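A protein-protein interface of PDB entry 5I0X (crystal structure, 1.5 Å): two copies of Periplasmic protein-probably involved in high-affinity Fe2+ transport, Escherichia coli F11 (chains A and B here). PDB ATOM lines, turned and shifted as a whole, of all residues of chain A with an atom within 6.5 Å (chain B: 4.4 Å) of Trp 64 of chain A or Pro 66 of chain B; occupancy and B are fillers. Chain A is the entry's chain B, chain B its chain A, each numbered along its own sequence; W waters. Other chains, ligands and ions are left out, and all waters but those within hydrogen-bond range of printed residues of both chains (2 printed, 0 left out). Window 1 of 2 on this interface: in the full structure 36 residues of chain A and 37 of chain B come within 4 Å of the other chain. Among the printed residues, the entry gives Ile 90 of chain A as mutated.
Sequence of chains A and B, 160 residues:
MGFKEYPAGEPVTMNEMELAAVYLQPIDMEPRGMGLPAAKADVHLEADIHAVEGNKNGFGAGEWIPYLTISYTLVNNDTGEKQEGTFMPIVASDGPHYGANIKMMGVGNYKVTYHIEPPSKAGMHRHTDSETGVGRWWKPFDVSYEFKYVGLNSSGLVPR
N of Tyr 67 of chain A lies within hydrogen-bond range of OH of Tyr 67 of chain B, at 2.9 Å.
The backbone carbonyl oxygen (O) of Pro 119 of chain B is in hydrogen-bond range of the backbone NH (N) of Met 124 of chain B (3.1 Å).
The backbone carbonyl oxygen of Ile 65 of chain B is in hydrogen-bond range of the side-chain hydroxyl of Tyr 98 of chain B (2.6 Å).
The side-chain hydroxyl of Tyr 98 of chain A sits at hydrogen-bond distance from the backbone NH of Leu 68 of chain A.
N of Ala 47 of chain A is in hydrogen-bond range of O of Tyr 98 of chain A (2.8 Å).
N of Leu 68 of chain B sits at hydrogen-bond distance from OH of Tyr 98 of chain B (3.0 Å).
The backbone NH of Tyr 67 of chain B lies within hydrogen-bond range of the side-chain hydroxyl of Tyr 98 of chain B (3.1 Å).
CG of Pro 66 of chain B touches CZ3 of Trp 64 of chain A, 3.9 Å away.
CE2 of Tyr 67 of chain B touches CH2 of Trp 64 of chain A, at 3.7 Å.
Trp 64 of chain A touches Met 124 of chain B (CH2 to CE, 3.8 Å).
Tyr 67 of chain A touches Trp 64 of chain B.
OH of Tyr 67 of chain A touches CE1 of Tyr 98 of chain B, 3.8 Å away.
CB of Pro 89 of chain A touches OH of Tyr 67 of chain B, 3.5 Å away.
Pro 89 of chain A touches Met 124 of chain B.
Val 91 of chain A touches Met 124 of chain B (CG1 to SD, 3.3 Å).
Met 124 of chain B touches Pro 96 of chain A (CE to CB, 3.9 Å).
Tyr 98 of chain A touches Tyr 67 of chain B.
Printed residues of chain B within 4 Å of Trp 64 of chain A: Pro 66, Tyr 67 and Met 124.
Pro 66 of chain B touches one residue of chain A.
Of the printed residues of chain A, Trp 64 of chain B touches Pro 66 and Tyr 67.
Of the printed residues of chain A, Tyr 67 of chain B touches Trp 64, Tyr 67, Pro 89 and Tyr 98.
Printed residues of chain B within 4 Å of Val 91 of chain A: Phe 59 (3.5 Å) and Met 124 (3.3 Å).
Printed residues of chain A within 4 Å of Met 124 of chain B: Trp 64, Pro 89, Val 91 and Pro 96.
Of the printed residues of chain A, Phe 59 of chain B touches Val 91.
The nearest printed residue of chain B that does not touch Trp 64 of chain A is Phe 59 of chain B (5.7 Å).
Of the 9 printed residues of chain B, 6 touch a printed residue of chain A.
Printed residues of chain B that touch a printed residue of chain A: Phe 59, Trp 64, Pro 66, Tyr 67, Tyr 98 and Met 124.
Of the 20 printed residues of chain A, 7 touch a printed residue of chain B.
Printed residues of chain A that touch a printed residue of chain B: Trp 64, Pro 66, Tyr 67, Pro 89, Val 91, Pro 96 and Tyr 98.
Among the printed residues, 13 pairs touch across the chains.
Among the printed residues, no Asp or Glu carboxylate lies within 4 Å of a Lys or Arg side-chain nitrogen of the other chain.
Trp 64 of chain A touches Pro 66 of chain B, and with the chains exchanged Pro 66 of chain A touches Trp 64 of chain B.
Trp 64 of chain A touches Tyr 67 of chain B, and with the chains exchanged Tyr 67 of chain A touches Trp 64 of chain B.
Tyr 67 of chain A touches its own counterpart, Tyr 67 of chain B.
Tyr 67 of chain A touches Tyr 98 of chain B, and with the chains exchanged Tyr 98 of chain A touches Tyr 67 of chain B.
Water W1 lies within hydrogen-bond range of the side-chain hydroxyl of Tyr 67 of chain B (2.5 Å) and the backbone carbonyl oxygen of Leu 68 of chain A (2.7 Å).
Water W2 bridges the side-chain hydroxyl (OH) of Tyr 67 of chain A and the backbone carbonyl oxygen (O) of Leu 68 of chain B.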
ATOM      1  N   ALA A  47     -20.479  11.156  21.474  1.00  0.00           N
ATOM      2  CA  ALA A  47     -21.654  10.475  22.021  1.00  0.00           C
ATOM      3  C   ALA A  47     -22.032   9.393  21.023  1.00  0.00           C
ATOM      4  O   ALA A  47     -22.228   9.681  19.815  1.00  0.00           O
ATOM      5  CB  ALA A  47     -22.811  11.438  22.198  1.00  0.00           C
ATOM      6  N   ASP A  48     -22.048   8.146  21.487  1.00  0.00           N
ATOM      7  CA  ASP A  48     -22.533   7.035  20.699  1.00  0.00           C
ATOM      8  C   ASP A  48     -23.910   6.689  21.199  1.00  0.00           C
ATOM      9  O   ASP A  48     -24.091   6.283  22.346  1.00  0.00           O
ATOM     10  CB  ASP A  48     -21.615   5.830  20.828  1.00  0.00           C
ATOM     11  CG  ASP A  48     -20.328   6.002  20.066  1.00  0.00           C
ATOM     12  OD1 ASP A  48     -20.350   6.576  18.952  1.00  0.00           O
ATOM     13  OD2 ASP A  48     -19.299   5.554  20.590  1.00  0.00           O
ATOM     14  N   ILE A  49     -24.876   6.869  20.319  1.00  0.00           N
ATOM     15  CA  ILE A  49     -26.297   6.740  20.682  1.00  0.00           C
ATOM     16  C   ILE A  49     -27.053   5.930  19.648  1.00  0.00           C
ATOM     17  O   ILE A  49     -27.102   6.324  18.468  1.00  0.00           O
ATOM     18  CB  ILE A  49     -26.958   8.130  20.825  1.00  0.00           C
ATOM     19  CG1 ILE A  49     -26.257   8.953  21.929  1.00  0.00           C
ATOM     20  CG2 ILE A  49     -28.450   7.980  21.145  1.00  0.00           C
ATOM     21  CD1 ILE A  49     -26.593  10.420  21.921  1.00  0.00           C
ATOM     22  N   HIS A  50     -27.654   4.819  20.082  1.00  0.00           N
ATOM     23  CA  HIS A  50     -28.381   3.918  19.174  1.00  0.00           C
ATOM     24  C   HIS A  50     -29.596   3.393  19.855  1.00  0.00           C
ATOM     25  O   HIS A  50     -29.589   3.203  21.075  1.00  0.00           O
ATOM     26  CB  HIS A  50     -27.494   2.754  18.719  1.00  0.00           C
ATOM     27  CG  HIS A  50     -26.258   3.218  18.011  1.00  0.00           C
ATOM     28  ND1 HIS A  50     -25.175   3.649  18.680  1.00  0.00           N
ATOM     29  CD2 HIS A  50     -26.004   3.427  16.661  1.00  0.00           C
ATOM     30  CE1 HIS A  50     -24.241   4.062  17.793  1.00  0.00           C
ATOM     31  NE2 HIS A  50     -24.758   3.951  16.561  1.00  0.00           N
ATOM     32  N   ALA A  51     -30.643   3.120  19.080  1.00  0.00           N
ATOM     33  CA  ALA A  51     -31.839   2.481  19.660  1.00  0.00           C
ATOM     34  C   ALA A  51     -31.512   1.098  20.201  1.00  0.00           C
ATOM     35  O   ALA A  51     -30.606   0.423  19.729  1.00  0.00           O
ATOM     36  CB  ALA A  51     -32.920   2.354  18.609  1.00  0.00           C
ATOM     37  N   PHE A  59     -37.370   3.547  15.499  1.00  0.00           N
ATOM     38  CA  PHE A  59     -36.014   3.070  15.207  1.00  0.00           C
ATOM     39  C   PHE A  59     -35.834   1.649  15.665  1.00  0.00           C
ATOM     40  O   PHE A  59     -36.230   1.300  16.773  1.00  0.00           O
ATOM     41  CB  PHE A  59     -34.948   3.996  15.828  1.00  0.00           C
ATOM     42  CG  PHE A  59     -35.025   5.383  15.310  1.00  0.00           C
ATOM     43  CD1 PHE A  59     -34.391   5.724  14.118  1.00  0.00           C
ATOM     44  CD2 PHE A  59     -35.772   6.350  15.970  1.00  0.00           C
ATOM     45  CE1 PHE A  59     -34.504   7.002  13.598  1.00  0.00           C
ATOM     46  CE2 PHE A  59     -35.894   7.635  15.447  1.00  0.00           C
ATOM     47  CZ  PHE A  59     -35.243   7.960  14.271  1.00  0.00           C
ATOM     48  N   GLY A  60     -35.261   0.829  14.800  1.00  0.00           N
ATOM     49  CA  GLY A  60     -34.979  -0.548  15.137  1.00  0.00           C
ATOM     50  C   GLY A  60     -33.713  -0.683  15.950  1.00  0.00           C
ATOM     51  O   GLY A  60     -32.861   0.203  15.953  1.00  0.00           O
ATOM     52  N   GLY A  62     -30.237  -1.064  17.379  1.00  0.00           N
ATOM     53  CA  GLY A  62     -28.907  -0.838  16.837  1.00  0.00           C
ATOM     54  C   GLY A  62     -28.810   0.367  15.922  1.00  0.00           C
ATOM     55  O   GLY A  62     -27.706   0.788  15.585  1.00  0.00           O
ATOM     56  N   GLU A  63     -29.959   0.893  15.492  1.00  0.00           N
ATOM     57  CA  GLU A  63     -29.968   2.016  14.553  1.00  0.00           C
ATOM     58  C   GLU A  63     -29.532   3.308  15.213  1.00  0.00           C
ATOM     59  O   GLU A  63     -29.878   3.575  16.352  1.00  0.00           O
ATOM     60  CB  GLU A  63     -31.325   2.165  13.880  1.00  0.00           C
ATOM     61  CG  GLU A  63     -31.613   1.007  12.945  1.00  0.00           C
ATOM     62  CD  GLU A  63     -33.057   0.948  12.499  1.00  0.00           C
ATOM     63  OE1 GLU A  63     -33.733   2.005  12.493  1.00  0.00           O
ATOM     64  OE2 GLU A  63     -33.510  -0.166  12.132  1.00  0.00           O
ATOM     65  N   TRP A  64     -28.754   4.108  14.488  1.00  0.00           N
ATOM     66  CA  TRP A  64     -28.363   5.432  14.982  1.00  0.00           C
ATOM     67  C   TRP A  64     -29.595   6.276  15.159  1.00  0.00           C
ATOM     68  O   TRP A  64     -30.554   6.157  14.371  1.00  0.00           O
ATOM     69  CB  TRP A  64     -27.432   6.084  13.966  1.00  0.00           C
ATOM     70  CG  TRP A  64     -26.785   7.341  14.474  1.00  0.00           C
ATOM     71  CD1 TRP A  64     -26.067   7.514  15.655  1.00  0.00           C
ATOM     72  CD2 TRP A  64     -26.795   8.642  13.819  1.00  0.00           C
ATOM     73  NE1 TRP A  64     -25.650   8.799  15.776  1.00  0.00           N
ATOM     74  CE2 TRP A  64     -26.045   9.535  14.685  1.00  0.00           C
ATOM     75  CE3 TRP A  64     -27.321   9.131  12.622  1.00  0.00           C
ATOM     76  CZ2 TRP A  64     -25.811  10.870  14.345  1.00  0.00           C
ATOM     77  CZ3 TRP A  64     -27.089  10.471  12.291  1.00  0.00           C
ATOM     78  CH2 TRP A  64     -26.364  11.318  13.140  1.00  0.00           C
ATOM     79  N   ILE A  65     -29.585   7.154  16.171  1.00  0.00           N
ATOM     80  CA  ILE A  65     -30.680   8.113  16.360  1.00  0.00           C
ATOM     81  C   ILE A  65     -30.234   9.456  15.778  1.00  0.00           C
ATOM     82  O   ILE A  65     -29.356  10.110  16.345  1.00  0.00           O
ATOM     83  CB  ILE A  65     -31.052   8.301  17.841  1.00  0.00           C
ATOM     84  CG1 ILE A  65     -31.278   6.936  18.556  1.00  0.00           C
ATOM     85  CG2 ILE A  65     -32.256   9.232  17.965  1.00  0.00           C
ATOM     86  CD1 ILE A  65     -32.400   6.092  17.949  1.00  0.00           C
ATOM     87  N   PRO A  66     -30.788   9.851  14.620  1.00  0.00           N
ATOM     88  CA  PRO A  66     -30.399  11.087  13.960  1.00  0.00           C
ATOM     89  C   PRO A  66     -31.185  12.283  14.448  1.00  0.00           C
ATOM     90  O   PRO A  66     -32.211  12.119  15.149  1.00  0.00           O
ATOM     91  CB  PRO A  66     -30.763  10.781  12.505  1.00  0.00           C
ATOM     92  CG  PRO A  66     -32.051  10.024  12.646  1.00  0.00           C
ATOM     93  CD  PRO A  66     -31.875   9.175  13.884  1.00  0.00           C
ATOM     94  N   TYR A  67     -30.687  13.478  14.144  1.00  0.00           N
ATOM     95  CA  TYR A  67     -31.379  14.745  14.417  1.00  0.00           C
ATOM     96  C   TYR A  67     -31.470  15.102  15.889  1.00  0.00           C
ATOM     97  O   TYR A  67     -32.284  15.946  16.279  1.00  0.00           O
ATOM     98  CB  TYR A  67     -32.762  14.806  13.745  1.00  0.00           C
ATOM     99  CG  TYR A  67     -32.682  14.852  12.232  1.00  0.00           C
ATOM    100  CD1 TYR A  67     -32.723  13.685  11.505  1.00  0.00           C
ATOM    101  CD2 TYR A  67     -32.520  16.047  11.545  1.00  0.00           C
ATOM    102  CE1 TYR A  67     -32.633  13.689  10.128  1.00  0.00           C
ATOM    103  CE2 TYR A  67     -32.448  16.064  10.147  1.00  0.00           C
ATOM    104  CZ  TYR A  67     -32.503  14.865   9.458  1.00  0.00           C
ATOM    105  OH  TYR A  67     -32.456  14.851   8.082  1.00  0.00           O
ATOM    106  N   LEU A  68     -30.633  14.476  16.716  1.00  0.00           N
ATOM    107  CA  LEU A  68     -30.572  14.895  18.117  1.00  0.00           C
ATOM    108  C   LEU A  68     -29.866  16.231  18.235  1.00  0.00           C
ATOM    109  O   LEU A  68     -28.985  16.543  17.436  1.00  0.00           O
ATOM    110  CB  LEU A  68     -29.857  13.859  18.973  1.00  0.00           C
ATOM    111  CG  LEU A  68     -30.531  12.490  19.012  1.00  0.00           C
ATOM    112  CD1 LEU A  68     -29.738  11.531  19.870  1.00  0.00           C
ATOM    113  CD2 LEU A  68     -31.963  12.588  19.560  1.00  0.00           C
ATOM    114  N   PRO A  89     -23.394  16.637  14.481  1.00  0.00           N
ATOM    115  CA  PRO A  89     -23.521  15.310  13.866  1.00  0.00           C
ATOM    116  C   PRO A  89     -22.331  15.084  12.934  1.00  0.00           C
ATOM    117  O   PRO A  89     -21.920  16.014  12.226  1.00  0.00           O
ATOM    118  CB  PRO A  89     -24.831  15.392  13.082  1.00  0.00           C
ATOM    119  CG  PRO A  89     -25.151  16.832  12.976  1.00  0.00           C
ATOM    120  CD  PRO A  89     -24.197  17.652  13.785  1.00  0.00           C
ATOM    121  N   ILE A  90     -21.779  13.871  12.963  1.00  0.00           N
ATOM    122  CA  ILE A  90     -20.509  13.593  12.282  1.00  0.00           C
ATOM    123  C   ILE A  90     -20.591  12.207  11.646  1.00  0.00           C
ATOM    124  O   ILE A  90     -21.174  11.281  12.207  1.00  0.00           O
ATOM    125  CB  ILE A  90     -19.336  13.578  13.301  1.00  0.00           C
ATOM    126  CG1 ILE A  90     -19.252  14.909  14.054  1.00  0.00           C
ATOM    127  CG2 ILE A  90     -18.020  13.318  12.572  1.00  0.00           C
ATOM    128  CD1 ILE A  90     -18.285  14.899  15.237  1.00  0.00           C
ATOM    129  N   VAL A  91     -20.037  12.066  10.451  1.00  0.00           N
ATOM    130  CA  VAL A  91     -19.801  10.721   9.910  1.00  0.00           C
ATOM    131  C   VAL A  91     -18.320  10.401   9.910  1.00  0.00           C
ATOM    132  O   VAL A  91     -17.460  11.259   9.683  1.00  0.00           O
ATOM    133  CB  VAL A  91     -20.353  10.532   8.474  1.00  0.00           C
ATOM    134  CG1 VAL A  91     -21.856  10.531   8.442  1.00  0.00           C
ATOM    135  CG2 VAL A  91     -19.823  11.546   7.481  1.00  0.00           C
ATOM    136  N   PRO A  96     -22.178   7.160  11.559  1.00  0.00           N
ATOM    137  CA  PRO A  96     -22.551   8.477  12.097  1.00  0.00           C
ATOM    138  C   PRO A  96     -22.529   8.462  13.619  1.00  0.00           C
ATOM    139  O   PRO A  96     -22.767   7.413  14.230  1.00  0.00           O
ATOM    140  CB  PRO A  96     -23.980   8.666  11.570  1.00  0.00           C
ATOM    141  CG  PRO A  96     -24.511   7.255  11.446  1.00  0.00           C
ATOM    142  CD  PRO A  96     -23.331   6.438  10.989  1.00  0.00           C
ATOM    143  N   HIS A  97     -22.216   9.613  14.206  1.00  0.00           N
ATOM    144  CA  HIS A  97     -22.191   9.814  15.657  1.00  0.00           C
ATOM    145  C   HIS A  97     -22.322  11.300  15.918  1.00  0.00           C
ATOM    146  O   HIS A  97     -22.577  12.079  15.009  1.00  0.00           O
ATOM    147  CB  HIS A  97     -20.905   9.227  16.262  1.00  0.00           C
ATOM    148  CG  HIS A  97     -19.641   9.860  15.747  1.00  0.00           C
ATOM    149  ND1 HIS A  97     -19.104   9.549  14.541  1.00  0.00           N
ATOM    150  CD2 HIS A  97     -18.820  10.808  16.314  1.00  0.00           C
ATOM    151  CE1 HIS A  97     -17.981  10.287  14.364  1.00  0.00           C
ATOM    152  NE2 HIS A  97     -17.793  11.035  15.446  1.00  0.00           N
ATOM    153  N   TYR A  98     -22.240  11.706  17.179  1.00  0.00           N
ATOM    154  CA  TYR A  98     -22.187  13.115  17.542  1.00  0.00           C
ATOM    155  C   TYR A  98     -20.902  13.360  18.285  1.00  0.00           C
ATOM    156  O   TYR A  98     -20.383  12.457  18.972  1.00  0.00           O
ATOM    157  CB  TYR A  98     -23.358  13.474  18.466  1.00  0.00           C
ATOM    158  CG  TYR A  98     -24.718  13.219  17.839  1.00  0.00           C
ATOM    159  CD1 TYR A  98     -25.316  14.186  17.041  1.00  0.00           C
ATOM    160  CD2 TYR A  98     -25.411  12.009  18.048  1.00  0.00           C
ATOM    161  CE1 TYR A  98     -26.576  13.976  16.483  1.00  0.00           C
ATOM    162  CE2 TYR A  98     -26.658  11.788  17.491  1.00  0.00           C
ATOM    163  CZ  TYR A  98     -27.229  12.767  16.702  1.00  0.00           C
ATOM    164  OH  TYR A  98     -28.447  12.539  16.132  1.00  0.00           O
ATOM    165  N   PHE B  59     -21.846   4.918   5.659  1.00  0.00           N
ATOM    166  CA  PHE B  59     -23.111   4.225   5.906  1.00  0.00           C
ATOM    167  C   PHE B  59     -23.083   2.789   5.441  1.00  0.00           C
ATOM    168  O   PHE B  59     -22.683   2.515   4.327  1.00  0.00           O
ATOM    169  CB  PHE B  59     -24.253   4.991   5.227  1.00  0.00           C
ATOM    170  CG  PHE B  59     -24.394   6.373   5.752  1.00  0.00           C
ATOM    171  CD1 PHE B  59     -25.012   6.596   6.975  1.00  0.00           C
ATOM    172  CD2 PHE B  59     -23.836   7.449   5.062  1.00  0.00           C
ATOM    173  CE1 PHE B  59     -25.096   7.874   7.501  1.00  0.00           C
ATOM    174  CE2 PHE B  59     -23.944   8.739   5.574  1.00  0.00           C
ATOM    175  CZ  PHE B  59     -24.565   8.938   6.800  1.00  0.00           C
ATOM    176  N   TRP B  64     -30.369   4.156   6.556  1.00  0.00           N
ATOM    177  CA  TRP B  64     -30.955   5.423   6.149  1.00  0.00           C
ATOM    178  C   TRP B  64     -29.871   6.478   5.986  1.00  0.00           C
ATOM    179  O   TRP B  64     -28.887   6.518   6.741  1.00  0.00           O
ATOM    180  CB  TRP B  64     -31.958   5.890   7.193  1.00  0.00           C
ATOM    181  CG  TRP B  64     -32.773   7.062   6.710  1.00  0.00           C
ATOM    182  CD1 TRP B  64     -33.536   7.155   5.523  1.00  0.00           C
ATOM    183  CD2 TRP B  64     -32.958   8.352   7.396  1.00  0.00           C
ATOM    184  NE1 TRP B  64     -34.145   8.377   5.439  1.00  0.00           N
ATOM    185  CE2 TRP B  64     -33.850   9.147   6.538  1.00  0.00           C
ATOM    186  CE3 TRP B  64     -32.505   8.910   8.608  1.00  0.00           C
ATOM    187  CZ2 TRP B  64     -34.273  10.430   6.902  1.00  0.00           C
ATOM    188  CZ3 TRP B  64     -32.917  10.215   8.940  1.00  0.00           C
ATOM    189  CH2 TRP B  64     -33.788  10.948   8.104  1.00  0.00           C
ATOM    190  N   ILE B  65     -30.021   7.315   4.967  1.00  0.00           N
ATOM    191  CA  ILE B  65     -29.102   8.449   4.773  1.00  0.00           C
ATOM    192  C   ILE B  65     -29.759   9.671   5.397  1.00  0.00           C
ATOM    193  O   ILE B  65     -30.759  10.184   4.880  1.00  0.00           O
ATOM    194  CB  ILE B  65     -28.796   8.718   3.283  1.00  0.00           C
ATOM    195  CG1 ILE B  65     -28.343   7.437   2.552  1.00  0.00           C
ATOM    196  CG2 ILE B  65     -27.765   9.846   3.166  1.00  0.00           C
ATOM    197  CD1 ILE B  65     -27.039   6.845   3.082  1.00  0.00           C
ATOM    198  N   PRO B  66     -29.238  10.122   6.550  1.00  0.00           N
ATOM    199  CA  PRO B  66     -29.793  11.256   7.272  1.00  0.00           C
ATOM    200  C   PRO B  66     -29.208  12.586   6.813  1.00  0.00           C
ATOM    201  O   PRO B  66     -28.171  12.635   6.153  1.00  0.00           O
ATOM    202  CB  PRO B  66     -29.320  10.991   8.707  1.00  0.00           C
ATOM    203  CG  PRO B  66     -27.947  10.423   8.503  1.00  0.00           C
ATOM    204  CD  PRO B  66     -28.038   9.587   7.235  1.00  0.00           C
ATOM    205  N   TYR B  67     -29.882  13.666   7.213  1.00  0.00           N
ATOM    206  CA  TYR B  67     -29.397  15.040   6.985  1.00  0.00           C
ATOM    207  C   TYR B  67     -29.379  15.485   5.522  1.00  0.00           C
ATOM    208  O   TYR B  67     -28.745  16.489   5.197  1.00  0.00           O
ATOM    209  CB  TYR B  67     -28.033  15.306   7.667  1.00  0.00           C
ATOM    210  CG  TYR B  67     -28.119  15.268   9.158  1.00  0.00           C
ATOM    211  CD1 TYR B  67     -28.418  16.396   9.899  1.00  0.00           C
ATOM    212  CD2 TYR B  67     -27.876  14.073   9.823  1.00  0.00           C
ATOM    213  CE1 TYR B  67     -28.501  16.331  11.282  1.00  0.00           C
ATOM    214  CE2 TYR B  67     -27.981  13.991  11.198  1.00  0.00           C
ATOM    215  CZ  TYR B  67     -28.284  15.117  11.911  1.00  0.00           C
ATOM    216  OH  TYR B  67     -28.350  15.010  13.289  1.00  0.00           O
ATOM    217  N   LEU B  68     -30.101  14.772   4.666  1.00  0.00           N
ATOM    218  CA  LEU B  68     -30.254  15.237   3.272  1.00  0.00           C
ATOM    219  C   LEU B  68     -31.133  16.466   3.183  1.00  0.00           C
ATOM    220  O   LEU B  68     -31.994  16.677   4.010  1.00  0.00           O
ATOM    221  CB  LEU B  68     -30.834  14.112   2.391  1.00  0.00           C
ATOM    222  CG  LEU B  68     -29.936  12.879   2.266  1.00  0.00           C
ATOM    223  CD1 LEU B  68     -30.599  11.794   1.421  1.00  0.00           C
ATOM    224  CD2 LEU B  68     -28.564  13.224   1.680  1.00  0.00           C
ATOM    225  N   TYR B  98     -38.019  10.792   4.150  1.00  0.00           N
ATOM    226  CA  TYR B  98     -38.251  12.202   3.839  1.00  0.00           C
ATOM    227  C   TYR B  98     -39.573  12.277   3.105  1.00  0.00           C
ATOM    228  O   TYR B  98     -39.922  11.354   2.359  1.00  0.00           O
ATOM    229  CB  TYR B  98     -37.153  12.746   2.911  1.00  0.00           C
ATOM    230  CG  TYR B  98     -35.787  12.700   3.505  1.00  0.00           C
ATOM    231  CD1 TYR B  98     -35.327  13.736   4.317  1.00  0.00           C
ATOM    232  CD2 TYR B  98     -34.954  11.588   3.287  1.00  0.00           C
ATOM    233  CE1 TYR B  98     -34.042  13.684   4.870  1.00  0.00           C
ATOM    234  CE2 TYR B  98     -33.676  11.531   3.837  1.00  0.00           C
ATOM    235  CZ  TYR B  98     -33.224  12.579   4.627  1.00  0.00           C
ATOM    236  OH  TYR B  98     -31.961  12.499   5.165  1.00  0.00           O
ATOM    237  N   PRO B 119     -25.425  15.640   3.090  1.00  0.00           N
ATOM    238  CA  PRO B 119     -25.625  15.950   4.507  1.00  0.00           C
ATOM    239  C   PRO B 119     -24.807  17.142   5.000  1.00  0.00           C
ATOM    240  O   PRO B 119     -25.192  17.733   6.001  1.00  0.00           O
ATOM    241  CB  PRO B 119     -25.174  14.659   5.195  1.00  0.00           C
ATOM    242  CG  PRO B 119     -25.566  13.601   4.213  1.00  0.00           C
ATOM    243  CD  PRO B 119     -25.168  14.200   2.881  1.00  0.00           C
ATOM    244  N   MET B 124     -24.070  18.212   8.824  1.00  0.00           N
ATOM    245  CA  MET B 124     -23.286  17.029   9.171  1.00  0.00           C
ATOM    246  C   MET B 124     -21.819  17.203   8.777  1.00  0.00           C
ATOM    247  O   MET B 124     -21.510  17.602   7.657  1.00  0.00           O
ATOM    248  CB  MET B 124     -23.887  15.776   8.542  1.00  0.00           C
ATOM    249  CG  MET B 124     -23.261  14.500   9.063  1.00  0.00           C
ATOM    250  SD  MET B 124     -24.050  13.015   8.416  1.00  0.00           S
ATOM    251  CE  MET B 124     -24.474  12.203   9.957  1.00  0.00           C
HETATM  252  O   HOH W   1     -28.828  16.953  14.768  1.00  0.00           O
HETATM  253  O   HOH W   2     -32.031  17.058   6.795  1.00  0.00           O
